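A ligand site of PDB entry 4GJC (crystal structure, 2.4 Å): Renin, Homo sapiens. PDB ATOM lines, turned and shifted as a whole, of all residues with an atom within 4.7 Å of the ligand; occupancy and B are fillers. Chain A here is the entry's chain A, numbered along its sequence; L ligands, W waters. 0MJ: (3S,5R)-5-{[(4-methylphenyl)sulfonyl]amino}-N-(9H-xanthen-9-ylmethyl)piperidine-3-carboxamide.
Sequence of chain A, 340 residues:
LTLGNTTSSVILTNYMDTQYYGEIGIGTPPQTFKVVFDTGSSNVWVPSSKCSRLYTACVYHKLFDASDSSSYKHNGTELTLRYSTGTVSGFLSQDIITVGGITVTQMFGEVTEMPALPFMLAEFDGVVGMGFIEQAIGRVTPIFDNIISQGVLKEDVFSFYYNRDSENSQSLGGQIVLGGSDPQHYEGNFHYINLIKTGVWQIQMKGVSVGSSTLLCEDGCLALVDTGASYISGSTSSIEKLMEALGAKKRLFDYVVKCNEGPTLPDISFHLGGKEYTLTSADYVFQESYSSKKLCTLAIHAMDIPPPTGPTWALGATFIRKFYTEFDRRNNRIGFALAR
Residues that only touch the ligand: Gln 19 (3.6 Å), Gly 40 (3.5 Å), Arg 82 (3.8 Å), Tyr 83 (3.3 Å), Pro 118 (3.7 Å), Phe 119 (3.97 Å), Phe 124 (3.7 Å), Val 127 (3.4 Å), Met 303 (3.6 Å), Ile 305 (3.4 Å) and Pro 306 (3.7 Å). 16 residues have an atom within 4 Å of the ligand: Gln 19, Asp 38, Gly 40, Arg 82, Tyr 83, Ser 84, Thr 85, Pro 118, Phe 119, Phe 124, Val 127, Asp 226, Gly 228, Met 303, Ile 305 and Pro 306. Along chain A the residues within 4 Å of the ligand span positions 19 to 306.
Water W3 bridges OD2 of Asp 226 (2.8 Å) and O28 of the ligand (2.8 Å). Water W2 bridges the backbone carbonyl oxygen (O) of Arg 82 (2.9 Å) and a nitrogen (N25) of the ligand (2.9 Å). Water W1 bridges the side-chain hydroxyl of Ser 84 (2.9 Å) and a nitrogen (N16) of the ligand (3.4 Å). Water W4 bridges the backbone carbonyl oxygen (O) of Gly 40 (2.9 Å) and an oxygen (O27) of the ligand (3.2 Å).
OD1 of Asp 38 sits close to OD1 of Asp 226 (2.7 Å). The side-chain carboxylate of Asp 38 lies close to the backbone NH of Gly 228. OD1 of Asp 38 lies within hydrogen-bond range of N of Gly 40 (3.1 Å). OD2 of Asp 38 sits at hydrogen-bond distance from OG of Ser 41 (2.6 Å). OD1 of Asp 226 is in hydrogen-bond range of N of Gly 228 (3.2 Å). The backbone NH (N) of Gly 40 lies within hydrogen-bond range of the side-chain carboxylate (OD1) of Asp 226, 3.2 Å away. The side-chain amide nitrogen (NE2) of Gln 19 is in hydrogen-bond range of the backbone carbonyl oxygen (O) of Leu 121 (2.9 Å).
OD1 of Asp 38 is in salt-bridge range of N21 of the ligand (2.7 Å). The backbone NH (N) of Ser 84 is in hydrogen-bond range of an oxygen (O24) of the ligand (3.2 Å). The side-chain hydroxyl (OG) of Ser 84 sits at hydrogen-bond distance from an oxygen (O24) of the ligand (2.8 Å). OD2 of Asp 226 is in salt-bridge range of N21 of the ligand (2.8 Å). The backbone carbonyl oxygen of Gly 228 sits at hydrogen-bond distance from a nitrogen (N16) of the ligand (3.0 Å). OG1 of Thr 85 is in hydrogen-bond range of O2 of the ligand (3.1 Å).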
ATOM      1  N   GLN A  19      21.759 -25.947 -27.848  1.00  0.00           N
ATOM      2  CA  GLN A  19      20.820 -24.862 -28.106  1.00  0.00           C
ATOM      3  C   GLN A  19      19.410 -25.400 -28.226  1.00  0.00           C
ATOM      4  O   GLN A  19      19.163 -26.327 -28.993  1.00  0.00           O
ATOM      5  CB  GLN A  19      21.222 -24.055 -29.358  1.00  0.00           C
ATOM      6  CG  GLN A  19      22.640 -23.420 -29.272  1.00  0.00           C
ATOM      7  CD  GLN A  19      23.073 -22.731 -30.526  1.00  0.00           C
ATOM      8  OE1 GLN A  19      22.265 -22.132 -31.227  1.00  0.00           O
ATOM      9  NE2 GLN A  19      24.378 -22.774 -30.829  1.00  0.00           N
ATOM     10  N   VAL A  36      15.791 -18.467 -27.763  1.00  0.00           N
ATOM     11  CA  VAL A  36      16.189 -19.238 -26.580  1.00  0.00           C
ATOM     12  C   VAL A  36      15.390 -18.639 -25.383  1.00  0.00           C
ATOM     13  O   VAL A  36      15.290 -17.416 -25.268  1.00  0.00           O
ATOM     14  CB  VAL A  36      17.733 -19.133 -26.405  1.00  0.00           C
ATOM     15  CG1 VAL A  36      18.150 -19.257 -24.940  1.00  0.00           C
ATOM     16  CG2 VAL A  36      18.407 -20.200 -27.220  1.00  0.00           C
ATOM     17  N   ASP A  38      15.490 -18.048 -21.705  1.00  0.00           N
ATOM     18  CA  ASP A  38      16.590 -17.929 -20.727  1.00  0.00           C
ATOM     19  C   ASP A  38      16.175 -17.467 -19.325  1.00  0.00           C
ATOM     20  O   ASP A  38      15.803 -16.311 -19.147  1.00  0.00           O
ATOM     21  CB  ASP A  38      17.677 -17.009 -21.355  1.00  0.00           C
ATOM     22  CG  ASP A  38      18.912 -16.731 -20.555  1.00  0.00           C
ATOM     23  OD1 ASP A  38      19.280 -17.579 -19.722  1.00  0.00           O
ATOM     24  OD2 ASP A  38      19.567 -15.688 -20.811  1.00  0.00           O
ATOM     25  N   GLY A  40      18.175 -17.129 -16.810  1.00  0.00           N
ATOM     26  CA  GLY A  40      19.283 -16.318 -16.330  1.00  0.00           C
ATOM     27  C   GLY A  40      19.302 -14.873 -16.792  1.00  0.00           C
ATOM     28  O   GLY A  40      20.244 -14.165 -16.485  1.00  0.00           O
ATOM     29  N   SER A  41      18.300 -14.418 -17.533  1.00  0.00           N
ATOM     30  CA  SER A  41      18.213 -13.016 -18.019  1.00  0.00           C
ATOM     31  C   SER A  41      16.746 -12.617 -18.107  1.00  0.00           C
ATOM     32  O   SER A  41      15.901 -13.498 -18.012  1.00  0.00           O
ATOM     33  CB  SER A  41      18.940 -12.839 -19.359  1.00  0.00           C
ATOM     34  OG  SER A  41      18.241 -13.483 -20.422  1.00  0.00           O
ATOM     35  N   ARG A  82      24.656  -8.019 -21.875  1.00  0.00           N
ATOM     36  CA  ARG A  82      25.899  -8.761 -21.699  1.00  0.00           C
ATOM     37  C   ARG A  82      25.620 -10.167 -21.267  1.00  0.00           C
ATOM     38  O   ARG A  82      24.924 -10.412 -20.280  1.00  0.00           O
ATOM     39  CB  ARG A  82      26.802  -8.030 -20.687  1.00  0.00           C
ATOM     40  CG  ARG A  82      27.316  -6.672 -21.187  1.00  0.00           C
ATOM     41  CD  ARG A  82      28.137  -5.878 -20.178  1.00  0.00           C
ATOM     42  NE  ARG A  82      28.574  -4.597 -20.752  1.00  0.00           N
ATOM     43  CZ  ARG A  82      27.886  -3.451 -20.703  1.00  0.00           C
ATOM     44  NH1 ARG A  82      26.715  -3.407 -20.079  1.00  0.00           N
ATOM     45  NH2 ARG A  82      28.359  -2.353 -21.268  1.00  0.00           N
ATOM     46  N   TYR A  83      26.154 -11.123 -22.044  1.00  0.00           N
ATOM     47  CA  TYR A  83      25.997 -12.544 -21.757  1.00  0.00           C
ATOM     48  C   TYR A  83      27.377 -13.118 -21.494  1.00  0.00           C
ATOM     49  O   TYR A  83      28.356 -12.366 -21.452  1.00  0.00           O
ATOM     50  CB  TYR A  83      25.187 -13.271 -22.881  1.00  0.00           C
ATOM     51  CG  TYR A  83      23.801 -12.680 -23.049  1.00  0.00           C
ATOM     52  CD1 TYR A  83      22.758 -13.039 -22.196  1.00  0.00           C
ATOM     53  CD2 TYR A  83      23.549 -11.707 -24.015  1.00  0.00           C
ATOM     54  CE1 TYR A  83      21.494 -12.473 -22.316  1.00  0.00           C
ATOM     55  CE2 TYR A  83      22.293 -11.105 -24.128  1.00  0.00           C
ATOM     56  CZ  TYR A  83      21.272 -11.507 -23.280  1.00  0.00           C
ATOM     57  OH  TYR A  83      20.021 -10.956 -23.410  1.00  0.00           O
ATOM     58  N   SER A  84      27.463 -14.401 -21.255  1.00  0.00           N
ATOM     59  CA  SER A  84      28.725 -15.022 -20.899  1.00  0.00           C
ATOM     60  C   SER A  84      29.700 -15.162 -22.079  1.00  0.00           C
ATOM     61  O   SER A  84      30.904 -15.040 -21.890  1.00  0.00           O
ATOM     62  CB  SER A  84      28.460 -16.365 -20.215  1.00  0.00           C
ATOM     63  OG  SER A  84      27.901 -17.290 -21.125  1.00  0.00           O
ATOM     64  N   THR A  85      29.152 -15.431 -23.273  1.00  0.00           N
ATOM     65  CA  THR A  85      29.858 -15.641 -24.542  1.00  0.00           C
ATOM     66  C   THR A  85      30.041 -14.361 -25.356  1.00  0.00           C
ATOM     67  O   THR A  85      30.877 -14.345 -26.268  1.00  0.00           O
ATOM     68  CB  THR A  85      29.083 -16.677 -25.401  1.00  0.00           C
ATOM     69  OG1 THR A  85      27.729 -16.218 -25.529  1.00  0.00           O
ATOM     70  CG2 THR A  85      29.067 -18.068 -24.779  1.00  0.00           C
ATOM     71  N   PRO A 118      30.003 -14.595 -30.459  1.00  0.00           N
ATOM     72  CA  PRO A 118      29.552 -15.964 -30.799  1.00  0.00           C
ATOM     73  C   PRO A 118      28.333 -16.102 -31.756  1.00  0.00           C
ATOM     74  O   PRO A 118      27.974 -17.217 -32.105  1.00  0.00           O
ATOM     75  CB  PRO A 118      29.169 -16.496 -29.406  1.00  0.00           C
ATOM     76  CG  PRO A 118      28.503 -15.295 -28.768  1.00  0.00           C
ATOM     77  CD  PRO A 118      29.283 -14.083 -29.279  1.00  0.00           C
ATOM     78  N   PHE A 119      27.669 -14.993 -32.115  1.00  0.00           N
ATOM     79  CA  PHE A 119      26.411 -15.051 -32.846  1.00  0.00           C
ATOM     80  C   PHE A 119      26.317 -15.780 -34.190  1.00  0.00           C
ATOM     81  O   PHE A 119      25.225 -16.167 -34.574  1.00  0.00           O
ATOM     82  CB  PHE A 119      25.640 -13.731 -32.797  1.00  0.00           C
ATOM     83  CG  PHE A 119      25.337 -13.353 -31.361  1.00  0.00           C
ATOM     84  CD1 PHE A 119      24.354 -14.034 -30.644  1.00  0.00           C
ATOM     85  CD2 PHE A 119      26.100 -12.401 -30.689  1.00  0.00           C
ATOM     86  CE1 PHE A 119      24.115 -13.717 -29.301  1.00  0.00           C
ATOM     87  CE2 PHE A 119      25.870 -12.112 -29.342  1.00  0.00           C
ATOM     88  CZ  PHE A 119      24.869 -12.770 -28.664  1.00  0.00           C
ATOM     89  N   LEU A 121      27.521 -18.754 -34.451  1.00  0.00           N
ATOM     90  CA  LEU A 121      27.373 -20.124 -33.912  1.00  0.00           C
ATOM     91  C   LEU A 121      25.950 -20.366 -33.430  1.00  0.00           C
ATOM     92  O   LEU A 121      25.596 -21.498 -33.097  1.00  0.00           O
ATOM     93  CB  LEU A 121      28.287 -20.334 -32.701  1.00  0.00           C
ATOM     94  CG  LEU A 121      29.777 -20.055 -32.834  1.00  0.00           C
ATOM     95  CD1 LEU A 121      30.386 -19.742 -31.448  1.00  0.00           C
ATOM     96  CD2 LEU A 121      30.514 -21.171 -33.554  1.00  0.00           C
ATOM     97  N   ALA A 122      25.162 -19.296 -33.350  1.00  0.00           N
ATOM     98  CA  ALA A 122      23.795 -19.337 -32.865  1.00  0.00           C
ATOM     99  C   ALA A 122      22.823 -19.763 -33.963  1.00  0.00           C
ATOM    100  O   ALA A 122      22.771 -19.163 -35.036  1.00  0.00           O
ATOM    101  CB  ALA A 122      23.414 -17.979 -32.276  1.00  0.00           C
ATOM    102  N   PHE A 124      19.626 -19.958 -33.141  1.00  0.00           N
ATOM    103  CA  PHE A 124      18.536 -19.075 -32.743  1.00  0.00           C
ATOM    104  C   PHE A 124      18.856 -17.636 -33.219  1.00  0.00           C
ATOM    105  O   PHE A 124      20.033 -17.302 -33.407  1.00  0.00           O
ATOM    106  CB  PHE A 124      18.336 -19.127 -31.189  1.00  0.00           C
ATOM    107  CG  PHE A 124      19.530 -18.670 -30.362  1.00  0.00           C
ATOM    108  CD1 PHE A 124      20.499 -19.578 -29.953  1.00  0.00           C
ATOM    109  CD2 PHE A 124      19.692 -17.339 -30.005  1.00  0.00           C
ATOM    110  CE1 PHE A 124      21.605 -19.159 -29.182  1.00  0.00           C
ATOM    111  CE2 PHE A 124      20.819 -16.909 -29.274  1.00  0.00           C
ATOM    112  CZ  PHE A 124      21.751 -17.830 -28.844  1.00  0.00           C
ATOM    113  N   VAL A 127      16.621 -13.855 -27.989  1.00  0.00           N
ATOM    114  CA  VAL A 127      16.463 -14.374 -26.637  1.00  0.00           C
ATOM    115  C   VAL A 127      15.197 -13.872 -25.996  1.00  0.00           C
ATOM    116  O   VAL A 127      14.853 -12.713 -26.190  1.00  0.00           O
ATOM    117  CB  VAL A 127      17.728 -14.013 -25.783  1.00  0.00           C
ATOM    118  CG1 VAL A 127      17.592 -14.449 -24.310  1.00  0.00           C
ATOM    119  CG2 VAL A 127      18.997 -14.587 -26.406  1.00  0.00           C
ATOM    120  N   LEU A 224      22.648 -21.102  -9.804  1.00  0.00           N
ATOM    121  CA  LEU A 224      21.739 -20.372 -10.712  1.00  0.00           C
ATOM    122  C   LEU A 224      21.116 -21.439 -11.644  1.00  0.00           C
ATOM    123  O   LEU A 224      21.852 -22.210 -12.274  1.00  0.00           O
ATOM    124  CB  LEU A 224      22.564 -19.318 -11.503  1.00  0.00           C
ATOM    125  CG  LEU A 224      21.804 -18.470 -12.529  1.00  0.00           C
ATOM    126  CD1 LEU A 224      20.846 -17.485 -11.844  1.00  0.00           C
ATOM    127  CD2 LEU A 224      22.780 -17.766 -13.445  1.00  0.00           C
ATOM    128  N   ASP A 226      19.708 -22.043 -14.782  1.00  0.00           N
ATOM    129  CA  ASP A 226      19.787 -21.290 -16.040  1.00  0.00           C
ATOM    130  C   ASP A 226      19.502 -22.087 -17.314  1.00  0.00           C
ATOM    131  O   ASP A 226      20.358 -22.782 -17.820  1.00  0.00           O
ATOM    132  CB  ASP A 226      21.182 -20.584 -16.128  1.00  0.00           C
ATOM    133  CG  ASP A 226      21.371 -19.583 -17.233  1.00  0.00           C
ATOM    134  OD1 ASP A 226      20.367 -19.233 -17.890  1.00  0.00           O
ATOM    135  OD2 ASP A 226      22.511 -19.114 -17.432  1.00  0.00           O
ATOM    136  N   GLY A 228      19.184 -20.911 -20.284  1.00  0.00           N
ATOM    137  CA  GLY A 228      19.952 -20.305 -21.366  1.00  0.00           C
ATOM    138  C   GLY A 228      21.392 -20.746 -21.419  1.00  0.00           C
ATOM    139  O   GLY A 228      22.121 -20.412 -22.358  1.00  0.00           O
ATOM    140  N   ALA A 229      21.835 -21.478 -20.395  1.00  0.00           N
ATOM    141  CA  ALA A 229      23.185 -21.980 -20.346  1.00  0.00           C
ATOM    142  C   ALA A 229      23.160 -23.420 -20.877  1.00  0.00           C
ATOM    143  O   ALA A 229      22.270 -24.200 -20.526  1.00  0.00           O
ATOM    144  CB  ALA A 229      23.686 -21.926 -18.906  1.00  0.00           C
ATOM    145  N   MET A 303      33.076 -20.905 -15.535  1.00  0.00           N
ATOM    146  CA  MET A 303      32.362 -19.666 -15.845  1.00  0.00           C
ATOM    147  C   MET A 303      32.345 -18.801 -14.598  1.00  0.00           C
ATOM    148  O   MET A 303      31.726 -19.170 -13.594  1.00  0.00           O
ATOM    149  CB  MET A 303      30.937 -19.943 -16.350  1.00  0.00           C
ATOM    150  CG  MET A 303      30.122 -18.712 -16.691  1.00  0.00           C
ATOM    151  SD  MET A 303      30.634 -17.959 -18.225  1.00  0.00           S
ATOM    152  CE  MET A 303      31.317 -16.483 -17.622  1.00  0.00           C
ATOM    153  N   ASP A 304      33.065 -17.683 -14.662  1.00  0.00           N
ATOM    154  CA  ASP A 304      33.112 -16.748 -13.555  1.00  0.00           C
ATOM    155  C   ASP A 304      32.026 -15.715 -13.787  1.00  0.00           C
ATOM    156  O   ASP A 304      32.161 -14.815 -14.626  1.00  0.00           O
ATOM    157  CB  ASP A 304      34.525 -16.144 -13.361  1.00  0.00           C
ATOM    158  CG  ASP A 304      35.565 -17.185 -12.998  1.00  0.00           C
ATOM    159  OD1 ASP A 304      36.554 -17.320 -13.735  1.00  0.00           O
ATOM    160  OD2 ASP A 304      35.374 -17.905 -11.985  1.00  0.00           O
ATOM    161  N   ILE A 305      30.893 -15.948 -13.129  1.00  0.00           N
ATOM    162  CA  ILE A 305      29.706 -15.086 -13.211  1.00  0.00           C
ATOM    163  C   ILE A 305      29.963 -13.910 -12.286  1.00  0.00           C
ATOM    164  O   ILE A 305      30.371 -14.127 -11.139  1.00  0.00           O
ATOM    165  CB  ILE A 305      28.386 -15.873 -12.945  1.00  0.00           C
ATOM    166  CG1 ILE A 305      28.150 -16.899 -14.085  1.00  0.00           C
ATOM    167  CG2 ILE A 305      27.165 -14.932 -12.773  1.00  0.00           C
ATOM    168  CD1 ILE A 305      27.568 -18.208 -13.707  1.00  0.00           C
ATOM    169  N   PRO A 306      29.863 -12.661 -12.790  1.00  0.00           N
ATOM    170  CA  PRO A 306      30.214 -11.512 -11.948  1.00  0.00           C
ATOM    171  C   PRO A 306      29.180 -11.168 -10.888  1.00  0.00           C
ATOM    172  O   PRO A 306      28.011 -11.490 -11.082  1.00  0.00           O
ATOM    173  CB  PRO A 306      30.380 -10.368 -12.958  1.00  0.00           C
ATOM    174  CG  PRO A 306      29.536 -10.742 -14.115  1.00  0.00           C
ATOM    175  CD  PRO A 306      29.470 -12.235 -14.157  1.00  0.00           C
HETATM  176  C1  0MJ L   1      23.917 -18.839 -25.200  1.00  0.00           C
HETATM  177  O2  0MJ L   1      24.862 -16.482 -26.555  1.00  0.00           O
HETATM  178  C3  0MJ L   1      23.207 -17.480 -25.060  1.00  0.00           C
HETATM  179  C4  0MJ L   1      24.610 -18.916 -26.584  1.00  0.00           C
HETATM  180  C5  0MJ L   1      23.750 -16.359 -25.724  1.00  0.00           C
HETATM  181  C6  0MJ L   1      25.064 -17.724 -27.193  1.00  0.00           C
HETATM  182  C7  0MJ L   1      24.999 -18.954 -24.067  1.00  0.00           C
HETATM  183  C8  0MJ L   1      24.801 -20.139 -27.263  1.00  0.00           C
HETATM  184  C9  0MJ L   1      22.053 -17.361 -24.258  1.00  0.00           C
HETATM  185  C10 0MJ L   1      23.130 -15.108 -25.605  1.00  0.00           C
HETATM  186  C11 0MJ L   1      25.689 -17.753 -28.470  1.00  0.00           C
HETATM  187  C12 0MJ L   1      21.449 -16.116 -24.099  1.00  0.00           C
HETATM  188  C13 0MJ L   1      25.432 -20.155 -28.541  1.00  0.00           C
HETATM  189  C14 0MJ L   1      21.996 -14.999 -24.792  1.00  0.00           C
HETATM  190  C15 0MJ L   1      25.893 -18.974 -29.144  1.00  0.00           C
HETATM  191  N16 0MJ L   1      24.493 -18.625 -22.724  1.00  0.00           N
HETATM  192  C17 0MJ L   1      24.770 -17.479 -22.013  1.00  0.00           C
HETATM  193  C18 0MJ L   1      24.097 -17.280 -20.665  1.00  0.00           C
HETATM  194  C19 0MJ L   1      24.512 -15.957 -19.938  1.00  0.00           C
HETATM  195  C20 0MJ L   1      22.262 -15.936 -18.689  1.00  0.00           C
HETATM  196  N21 0MJ L   1      21.901 -17.189 -19.380  1.00  0.00           N
HETATM  197  C22 0MJ L   1      23.811 -15.875 -18.552  1.00  0.00           C
HETATM  198  C23 0MJ L   1      22.532 -17.383 -20.721  1.00  0.00           C
HETATM  199  O24 0MJ L   1      25.527 -16.598 -22.430  1.00  0.00           O
HETATM  200  N25 0MJ L   1      24.236 -14.691 -17.824  1.00  0.00           N
HETATM  201  S26 0MJ L   1      25.156 -14.722 -16.465  1.00  0.00           S
HETATM  202  O27 0MJ L   1      24.471 -13.944 -15.434  1.00  0.00           O
HETATM  203  O28 0MJ L   1      25.511 -16.091 -16.142  1.00  0.00           O
HETATM  204  C29 0MJ L   1      26.596 -13.856 -17.067  1.00  0.00           C
HETATM  205  C30 0MJ L   1      26.485 -12.528 -17.544  1.00  0.00           C
HETATM  206  C31 0MJ L   1      28.887 -12.470 -17.963  1.00  0.00           C
HETATM  207  C32 0MJ L   1      28.994 -13.787 -17.477  1.00  0.00           C
HETATM  208  C33 0MJ L   1      27.628 -11.838 -17.995  1.00  0.00           C
HETATM  209  C34 0MJ L   1      27.859 -14.481 -17.028  1.00  0.00           C
HETATM  210  C35 0MJ L   1      30.138 -11.727 -18.462  1.00  0.00           C
HETATM  211  O   HOH W   1      26.287 -19.389 -19.896  1.00  0.00           O
HETATM  212  O   HOH W   2      23.135 -12.113 -18.711  1.00  0.00           O
HETATM  213  O   HOH W   3      25.150 -18.892 -16.472  1.00  0.00           O
HETATM  214  O   HOH W   4      21.627 -14.124 -13.979  1.00  0.00           O
